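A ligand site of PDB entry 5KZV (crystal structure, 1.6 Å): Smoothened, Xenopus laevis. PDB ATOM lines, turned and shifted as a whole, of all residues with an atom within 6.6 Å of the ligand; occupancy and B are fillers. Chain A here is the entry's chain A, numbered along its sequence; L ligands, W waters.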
ATOM      1  N   ASP A  41      21.354 -34.791  22.739  1.00  0.00           N
ATOM      2  CA  ASP A  41      21.951 -34.501  21.443  1.00  0.00           C
ATOM      3  C   ASP A  41      23.478 -34.296  21.547  1.00  0.00           C
ATOM      4  O   ASP A  41      24.137 -34.064  20.530  1.00  0.00           O
ATOM      5  CB  ASP A  41      21.295 -33.251  20.809  1.00  0.00           C
ATOM      6  CG  ASP A  41      21.565 -31.953  21.596  1.00  0.00           C
ATOM      7  OD1 ASP A  41      22.097 -32.001  22.730  1.00  0.00           O
ATOM      8  OD2 ASP A  41      21.200 -30.868  21.073  1.00  0.00           O
ATOM      9  N   LYS A  51      26.184 -27.200  19.854  1.00  0.00           N
ATOM     10  CA  LYS A  51      24.720 -27.198  19.842  1.00  0.00           C
ATOM     11  C   LYS A  51      24.189 -25.882  20.414  1.00  0.00           C
ATOM     12  O   LYS A  51      23.252 -25.287  19.868  1.00  0.00           O
ATOM     13  CB  LYS A  51      24.136 -28.368  20.649  1.00  0.00           C
ATOM     14  CG  LYS A  51      24.495 -29.781  20.122  1.00  0.00           C
ATOM     15  CD  LYS A  51      23.924 -30.038  18.741  1.00  0.00           C
ATOM     16  CE  LYS A  51      24.524 -31.307  18.167  1.00  0.00           C
ATOM     17  NZ  LYS A  51      24.170 -31.492  16.743  1.00  0.00           N
ATOM     18  N   LEU A  52      24.794 -25.394  21.488  1.00  0.00           N
ATOM     19  CA  LEU A  52      24.400 -24.085  22.034  1.00  0.00           C
ATOM     20  C   LEU A  52      24.618 -22.980  21.007  1.00  0.00           C
ATOM     21  O   LEU A  52      23.855 -22.018  20.958  1.00  0.00           O
ATOM     22  CB  LEU A  52      25.168 -23.787  23.321  1.00  0.00           C
ATOM     23  CG  LEU A  52      24.700 -24.629  24.513  1.00  0.00           C
ATOM     24  CD1 LEU A  52      25.597 -24.369  25.731  1.00  0.00           C
ATOM     25  CD2 LEU A  52      23.206 -24.392  24.836  1.00  0.00           C
ATOM     26  N   LEU A  54      24.239 -23.276  17.785  1.00  0.00           N
ATOM     27  CA  LEU A  54      23.067 -23.335  16.910  1.00  0.00           C
ATOM     28  C   LEU A  54      21.861 -22.658  17.569  1.00  0.00           C
ATOM     29  O   LEU A  54      21.143 -21.878  16.933  1.00  0.00           O
ATOM     30  CB  LEU A  54      22.724 -24.775  16.572  1.00  0.00           C
ATOM     31  CG  LEU A  54      23.555 -25.399  15.459  1.00  0.00           C
ATOM     32  CD1 LEU A  54      23.263 -26.885  15.374  1.00  0.00           C
ATOM     33  CD2 LEU A  54      23.234 -24.732  14.131  1.00  0.00           C
ATOM     34  N   TRP A  55      21.610 -22.989  18.842  1.00  0.00           N
ATOM     35  CA  TRP A  55      20.511 -22.362  19.574  1.00  0.00           C
ATOM     36  C   TRP A  55      20.621 -20.848  19.632  1.00  0.00           C
ATOM     37  O   TRP A  55      19.594 -20.134  19.643  1.00  0.00           O
ATOM     38  CB  TRP A  55      20.431 -22.911  21.003  1.00  0.00           C
ATOM     39  CG  TRP A  55      19.815 -24.261  21.144  1.00  0.00           C
ATOM     40  CD1 TRP A  55      20.450 -25.431  21.496  1.00  0.00           C
ATOM     41  CD2 TRP A  55      18.435 -24.593  20.954  1.00  0.00           C
ATOM     42  NE1 TRP A  55      19.549 -26.449  21.544  1.00  0.00           N
ATOM     43  CE2 TRP A  55      18.308 -25.976  21.204  1.00  0.00           C
ATOM     44  CE3 TRP A  55      17.299 -23.854  20.597  1.00  0.00           C
ATOM     45  CZ2 TRP A  55      17.077 -26.641  21.106  1.00  0.00           C
ATOM     46  CZ3 TRP A  55      16.081 -24.521  20.492  1.00  0.00           C
ATOM     47  CH2 TRP A  55      15.978 -25.903  20.744  1.00  0.00           C
ATOM     48  N   SER A  56      21.863 -20.339  19.666  1.00  0.00           N
ATOM     49  CA  SER A  56      22.131 -18.906  19.713  1.00  0.00           C
ATOM     50  C   SER A  56      21.536 -18.077  18.578  1.00  0.00           C
ATOM     51  O   SER A  56      21.503 -16.845  18.662  1.00  0.00           O
ATOM     52  CB  SER A  56      23.634 -18.675  19.742  1.00  0.00           C
ATOM     53  OG  SER A  56      24.110 -18.905  21.058  1.00  0.00           O
ATOM     54  N   GLY A  57      21.051 -18.727  17.523  1.00  0.00           N
ATOM     55  CA  GLY A  57      20.280 -18.024  16.515  1.00  0.00           C
ATOM     56  C   GLY A  57      19.042 -17.353  17.092  1.00  0.00           C
ATOM     57  O   GLY A  57      18.545 -16.343  16.560  1.00  0.00           O
ATOM     58  N   LEU A  58      18.539 -17.886  18.207  1.00  0.00           N
ATOM     59  CA  LEU A  58      17.395 -17.276  18.882  1.00  0.00           C
ATOM     60  C   LEU A  58      17.721 -15.968  19.618  1.00  0.00           C
ATOM     61  O   LEU A  58      16.831 -15.351  20.228  1.00  0.00           O
ATOM     62  CB  LEU A  58      16.780 -18.273  19.872  1.00  0.00           C
ATOM     63  CG  LEU A  58      15.960 -19.409  19.259  1.00  0.00           C
ATOM     64  CD1 LEU A  58      15.640 -20.471  20.311  1.00  0.00           C
ATOM     65  CD2 LEU A  58      14.684 -18.854  18.643  1.00  0.00           C
ATOM     66  N   ARG A  59      18.989 -15.536  19.595  1.00  0.00           N
ATOM     67  CA  ARG A  59      19.313 -14.206  20.156  1.00  0.00           C
ATOM     68  C   ARG A  59      18.560 -13.124  19.379  1.00  0.00           C
ATOM     69  O   ARG A  59      18.256 -12.050  19.918  1.00  0.00           O
ATOM     70  CB  ARG A  59      20.808 -13.909  20.098  1.00  0.00           C
ATOM     71  CG  ARG A  59      21.659 -14.608  21.140  1.00  0.00           C
ATOM     72  CD  ARG A  59      23.119 -14.235  20.889  1.00  0.00           C
ATOM     73  NE  ARG A  59      24.031 -14.784  21.884  1.00  0.00           N
ATOM     74  CZ  ARG A  59      24.402 -14.140  22.985  1.00  0.00           C
ATOM     75  NH1 ARG A  59      23.926 -12.922  23.235  1.00  0.00           N
ATOM     76  NH2 ARG A  59      25.242 -14.708  23.833  1.00  0.00           N
ATOM     77  N   ASN A  60      18.268 -13.396  18.110  1.00  0.00           N
ATOM     78  CA  ASN A  60      17.518 -12.466  17.266  1.00  0.00           C
ATOM     79  C   ASN A  60      16.015 -12.462  17.553  1.00  0.00           C
ATOM     80  O   ASN A  60      15.250 -11.817  16.843  1.00  0.00           O
ATOM     81  CB  ASN A  60      17.766 -12.773  15.801  1.00  0.00           C
ATOM     82  CG  ASN A  60      19.135 -12.341  15.342  1.00  0.00           C
ATOM     83  OD1 ASN A  60      19.635 -11.276  15.733  1.00  0.00           O
ATOM     84  ND2 ASN A  60      19.762 -13.152  14.498  1.00  0.00           N
ATOM     85  N   ALA A  61      15.596 -13.203  18.572  1.00  0.00           N
ATOM     86  CA  ALA A  61      14.202 -13.195  19.020  1.00  0.00           C
ATOM     87  C   ALA A  61      14.206 -13.036  20.545  1.00  0.00           C
ATOM     88  O   ALA A  61      14.077 -14.014  21.261  1.00  0.00           O
ATOM     89  CB  ALA A  61      13.479 -14.478  18.603  1.00  0.00           C
ATOM     90  N   TYR A  76      21.886 -28.204  29.180  1.00  0.00           N
ATOM     91  CA  TYR A  76      23.150 -28.435  28.485  1.00  0.00           C
ATOM     92  C   TYR A  76      24.375 -28.297  29.399  1.00  0.00           C
ATOM     93  O   TYR A  76      25.390 -28.966  29.167  1.00  0.00           O
ATOM     94  CB  TYR A  76      23.319 -27.464  27.309  1.00  0.00           C
ATOM     95  CG  TYR A  76      22.541 -27.881  26.085  1.00  0.00           C
ATOM     96  CD1 TYR A  76      21.201 -27.526  25.921  1.00  0.00           C
ATOM     97  CD2 TYR A  76      23.152 -28.649  25.080  1.00  0.00           C
ATOM     98  CE1 TYR A  76      20.485 -27.901  24.800  1.00  0.00           C
ATOM     99  CE2 TYR A  76      22.437 -29.028  23.946  1.00  0.00           C
ATOM    100  CZ  TYR A  76      21.099 -28.658  23.814  1.00  0.00           C
ATOM    101  OH  TYR A  76      20.366 -29.019  22.703  1.00  0.00           O
ATOM    102  N   ILE A 102       8.051 -20.447  17.919  1.00  0.00           N
ATOM    103  CA  ILE A 102       8.682 -20.504  16.607  1.00  0.00           C
ATOM    104  C   ILE A 102       9.553 -21.766  16.470  1.00  0.00           C
ATOM    105  O   ILE A 102       9.708 -22.334  15.376  1.00  0.00           O
ATOM    106  CB  ILE A 102       9.524 -19.229  16.348  1.00  0.00           C
ATOM    107  CG1 ILE A 102      10.026 -19.182  14.901  1.00  0.00           C
ATOM    108  CG2 ILE A 102      10.671 -19.136  17.358  1.00  0.00           C
ATOM    109  CD1 ILE A 102       8.919 -19.148  13.871  1.00  0.00           C
ATOM    110  N   VAL A 103      10.096 -22.232  17.593  1.00  0.00           N
ATOM    111  CA  VAL A 103      10.912 -23.444  17.608  1.00  0.00           C
ATOM    112  C   VAL A 103      10.096 -24.660  17.158  1.00  0.00           C
ATOM    113  O   VAL A 103      10.549 -25.497  16.353  1.00  0.00           O
ATOM    114  CB  VAL A 103      11.495 -23.708  18.992  1.00  0.00           C
ATOM    115  CG1 VAL A 103      12.198 -25.061  19.040  1.00  0.00           C
ATOM    116  CG2 VAL A 103      12.453 -22.585  19.368  1.00  0.00           C
ATOM    117  N   ALA A 104       8.876 -24.752  17.669  1.00  0.00           N
ATOM    118  CA  ALA A 104       7.978 -25.851  17.312  1.00  0.00           C
ATOM    119  C   ALA A 104       7.559 -25.794  15.851  1.00  0.00           C
ATOM    120  O   ALA A 104       7.418 -26.838  15.214  1.00  0.00           O
ATOM    121  CB  ALA A 104       6.753 -25.858  18.204  1.00  0.00           C
ATOM    122  N   GLU A 106       9.330 -24.240  13.319  1.00  0.00           N
ATOM    123  CA  GLU A 106      10.490 -24.290  12.439  1.00  0.00           C
ATOM    124  C   GLU A 106      11.044 -25.695  12.270  1.00  0.00           C
ATOM    125  O   GLU A 106      11.594 -26.028  11.231  1.00  0.00           O
ATOM    126  CB  GLU A 106      11.604 -23.379  12.953  1.00  0.00           C
ATOM    127  CG  GLU A 106      11.436 -21.906  12.605  1.00  0.00           C
ATOM    128  CD  GLU A 106      12.353 -21.464  11.456  1.00  0.00           C
ATOM    129  OE1 GLU A 106      11.929 -21.583  10.281  1.00  0.00           O
ATOM    130  OE2 GLU A 106      13.495 -21.010  11.742  1.00  0.00           O
ATOM    131  N   ARG A 107      10.921 -26.520  13.304  1.00  0.00           N
ATOM    132  CA  ARG A 107      11.565 -27.839  13.286  1.00  0.00           C
ATOM    133  C   ARG A 107      10.937 -28.800  14.273  1.00  0.00           C
ATOM    134  O   ARG A 107      10.752 -29.996  13.985  1.00  0.00           O
ATOM    135  CB  ARG A 107      13.062 -27.699  13.576  1.00  0.00           C
ATOM    136  CG  ARG A 107      13.749 -29.026  13.800  1.00  0.00           C
ATOM    137  CD  ARG A 107      15.264 -28.912  14.003  1.00  0.00           C
ATOM    138  NE  ARG A 107      15.777 -30.266  14.215  1.00  0.00           N
ATOM    139  CZ  ARG A 107      16.211 -31.068  13.245  1.00  0.00           C
ATOM    140  NH1 ARG A 107      16.263 -30.643  11.990  1.00  0.00           N
ATOM    141  NH2 ARG A 107      16.617 -32.289  13.544  1.00  0.00           N
ATOM    142  N   GLY A 108      10.627 -28.287  15.453  1.00  0.00           N
ATOM    143  CA  GLY A 108      10.099 -29.092  16.542  1.00  0.00           C
ATOM    144  C   GLY A 108      11.076 -29.177  17.710  1.00  0.00           C
ATOM    145  O   GLY A 108      12.295 -29.200  17.527  1.00  0.00           O
ATOM    146  N   TRP A 109      10.539 -29.184  18.921  1.00  0.00           N
ATOM    147  CA  TRP A 109      11.370 -29.388  20.114  1.00  0.00           C
ATOM    148  C   TRP A 109      11.940 -30.800  20.148  1.00  0.00           C
ATOM    149  O   TRP A 109      11.202 -31.769  19.927  1.00  0.00           O
ATOM    150  CB  TRP A 109      10.565 -29.140  21.403  1.00  0.00           C
ATOM    151  CG  TRP A 109      10.115 -27.748  21.612  1.00  0.00           C
ATOM    152  CD1 TRP A 109       8.866 -27.243  21.382  1.00  0.00           C
ATOM    153  CD2 TRP A 109      10.887 -26.685  22.177  1.00  0.00           C
ATOM    154  NE1 TRP A 109       8.826 -25.914  21.740  1.00  0.00           N
ATOM    155  CE2 TRP A 109      10.051 -25.547  22.242  1.00  0.00           C
ATOM    156  CE3 TRP A 109      12.214 -26.571  22.634  1.00  0.00           C
ATOM    157  CZ2 TRP A 109      10.490 -24.322  22.707  1.00  0.00           C
ATOM    158  CZ3 TRP A 109      12.652 -25.343  23.113  1.00  0.00           C
ATOM    159  CH2 TRP A 109      11.790 -24.237  23.148  1.00  0.00           C
ATOM    160  N   PRO A 110      13.243 -30.938  20.439  1.00  0.00           N
ATOM    161  CA  PRO A 110      13.752 -32.301  20.645  1.00  0.00           C
ATOM    162  C   PRO A 110      13.050 -32.939  21.836  1.00  0.00           C
ATOM    163  O   PRO A 110      12.551 -32.208  22.690  1.00  0.00           O
ATOM    164  CB  PRO A 110      15.234 -32.073  20.932  1.00  0.00           C
ATOM    165  CG  PRO A 110      15.538 -30.673  20.467  1.00  0.00           C
ATOM    166  CD  PRO A 110      14.278 -29.909  20.655  1.00  0.00           C
ATOM    167  N   PHE A 112      14.027 -34.339  24.549  1.00  0.00           N
ATOM    168  CA  PHE A 112      14.576 -33.994  25.859  1.00  0.00           C
ATOM    169  C   PHE A 112      14.331 -32.520  26.243  1.00  0.00           C
ATOM    170  O   PHE A 112      14.754 -32.072  27.308  1.00  0.00           O
ATOM    171  CB  PHE A 112      16.085 -34.333  25.927  1.00  0.00           C
ATOM    172  CG  PHE A 112      16.955 -33.523  24.994  1.00  0.00           C
ATOM    173  CD1 PHE A 112      17.119 -33.905  23.669  1.00  0.00           C
ATOM    174  CD2 PHE A 112      17.629 -32.403  25.469  1.00  0.00           C
ATOM    175  CE1 PHE A 112      17.936 -33.143  22.819  1.00  0.00           C
ATOM    176  CE2 PHE A 112      18.441 -31.645  24.627  1.00  0.00           C
ATOM    177  CZ  PHE A 112      18.589 -32.016  23.298  1.00  0.00           C
ATOM    178  N   LEU A 113      13.648 -31.779  25.363  1.00  0.00           N
ATOM    179  CA  LEU A 113      13.232 -30.406  25.632  1.00  0.00           C
ATOM    180  C   LEU A 113      11.718 -30.232  25.448  1.00  0.00           C
ATOM    181  O   LEU A 113      11.228 -29.111  25.217  1.00  0.00           O
ATOM    182  CB  LEU A 113      13.989 -29.415  24.741  1.00  0.00           C
ATOM    183  CG  LEU A 113      15.471 -29.263  25.079  1.00  0.00           C
ATOM    184  CD1 LEU A 113      16.247 -28.550  23.975  1.00  0.00           C
ATOM    185  CD2 LEU A 113      15.638 -28.508  26.399  1.00  0.00           C
HETATM  186  C1  LIG L   1      19.645 -26.983  18.009  1.00  0.00           C
HETATM  187  O1  LIG L   1      19.738 -30.669  18.851  1.00  0.00           O
HETATM  188  C2  LIG L   1      20.236 -28.388  18.168  1.00  0.00           C
HETATM  189  O2  LIG L   1      16.040 -20.932  13.361  1.00  0.00           O
HETATM  190  C3  LIG L   1      19.164 -29.364  18.656  1.00  0.00           C
HETATM  191  C4  LIG L   1      18.052 -29.453  17.617  1.00  0.00           C
HETATM  192  C5  LIG L   1      17.526 -28.070  17.337  1.00  0.00           C
HETATM  193  C6  LIG L   1      16.178 -27.893  17.371  1.00  0.00           C
HETATM  194  C7  LIG L   1      15.507 -26.569  17.032  1.00  0.00           C
HETATM  195  C8  LIG L   1      16.460 -25.685  16.251  1.00  0.00           C
HETATM  196  C9  LIG L   1      17.777 -25.631  17.019  1.00  0.00           C
HETATM  197  C10 LIG L   1      18.492 -26.972  17.005  1.00  0.00           C
HETATM  198  C11 LIG L   1      18.700 -24.517  16.510  1.00  0.00           C
HETATM  199  C12 LIG L   1      18.014 -23.146  16.444  1.00  0.00           C
HETATM  200  C13 LIG L   1      16.766 -23.215  15.560  1.00  0.00           C
HETATM  201  C14 LIG L   1      15.862 -24.287  16.147  1.00  0.00           C
HETATM  202  C15 LIG L   1      14.534 -24.159  15.407  1.00  0.00           C
HETATM  203  C16 LIG L   1      14.452 -22.659  15.130  1.00  0.00           C
HETATM  204  C17 LIG L   1      15.789 -22.034  15.565  1.00  0.00           C
HETATM  205  C18 LIG L   1      17.149 -23.584  14.129  1.00  0.00           C
HETATM  206  C19 LIG L   1      19.035 -27.254  15.604  1.00  0.00           C
HETATM  207  C20 LIG L   1      16.119 -20.737  14.786  1.00  0.00           C
HETATM  208  C21 LIG L   1      17.488 -20.139  15.127  1.00  0.00           C
HETATM  209  C22 LIG L   1      15.075 -19.687  15.149  1.00  0.00           C
HETATM  210  C23 LIG L   1      15.329 -18.361  14.452  1.00  0.00           C
HETATM  211  C24 LIG L   1      14.111 -17.449  14.570  1.00  0.00           C
HETATM  212  C25 LIG L   1      14.374 -16.132  13.861  1.00  0.00           C
HETATM  213  C26 LIG L   1      15.405 -15.307  14.623  1.00  0.00           C
HETATM  214  C27 LIG L   1      13.080 -15.363  13.676  1.00  0.00           C
HETATM  215  O   HOH W   1      18.267 -33.200  18.684  1.00  0.00           O
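OD2 of Asp 41 sits at hydrogen-bond distance from O1 of the ligand (2.7 Å). The side-chain carboxylate (OE2) of Glu 106 sits at hydrogen-bond distance from an oxygen (O2) of the ligand, at 3.0 Å.
Leu 54 touches the ligand (O to C12, 3.4 Å). Trp 55 touches the ligand. Gly 57 touches the ligand. Leu 58 touches the ligand (CD2 to C22, 3.6 Å). CB of Asn 60 touches C26 of the ligand, at 3.7 Å. CD of Arg 107 touches C6 of the ligand, 3.6 Å away. Pro 110 touches the ligand. Hydrophobic or aromatic side chains that line the ligand: Trp 55, Leu 58 and Pro 110. Nine residues have an atom within 4 Å of the ligand: Asp 41, Leu 54, Trp 55, Gly 57, Leu 58, Asn 60, Glu 106, Arg 107 and Pro 110. The nearest printed residue that does not touch the ligand is Lys 51 (4.1 Å).
The indole nitrogen (NE1) of Trp 55 is in hydrogen-bond range of the side-chain hydroxyl (OH) of Tyr 76 (2.9 Å). The side-chain carboxylate (OD2) of Asp 41 lies within hydrogen-bond range of the side-chain hydroxyl (OH) of Tyr 76 (2.6 Å).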
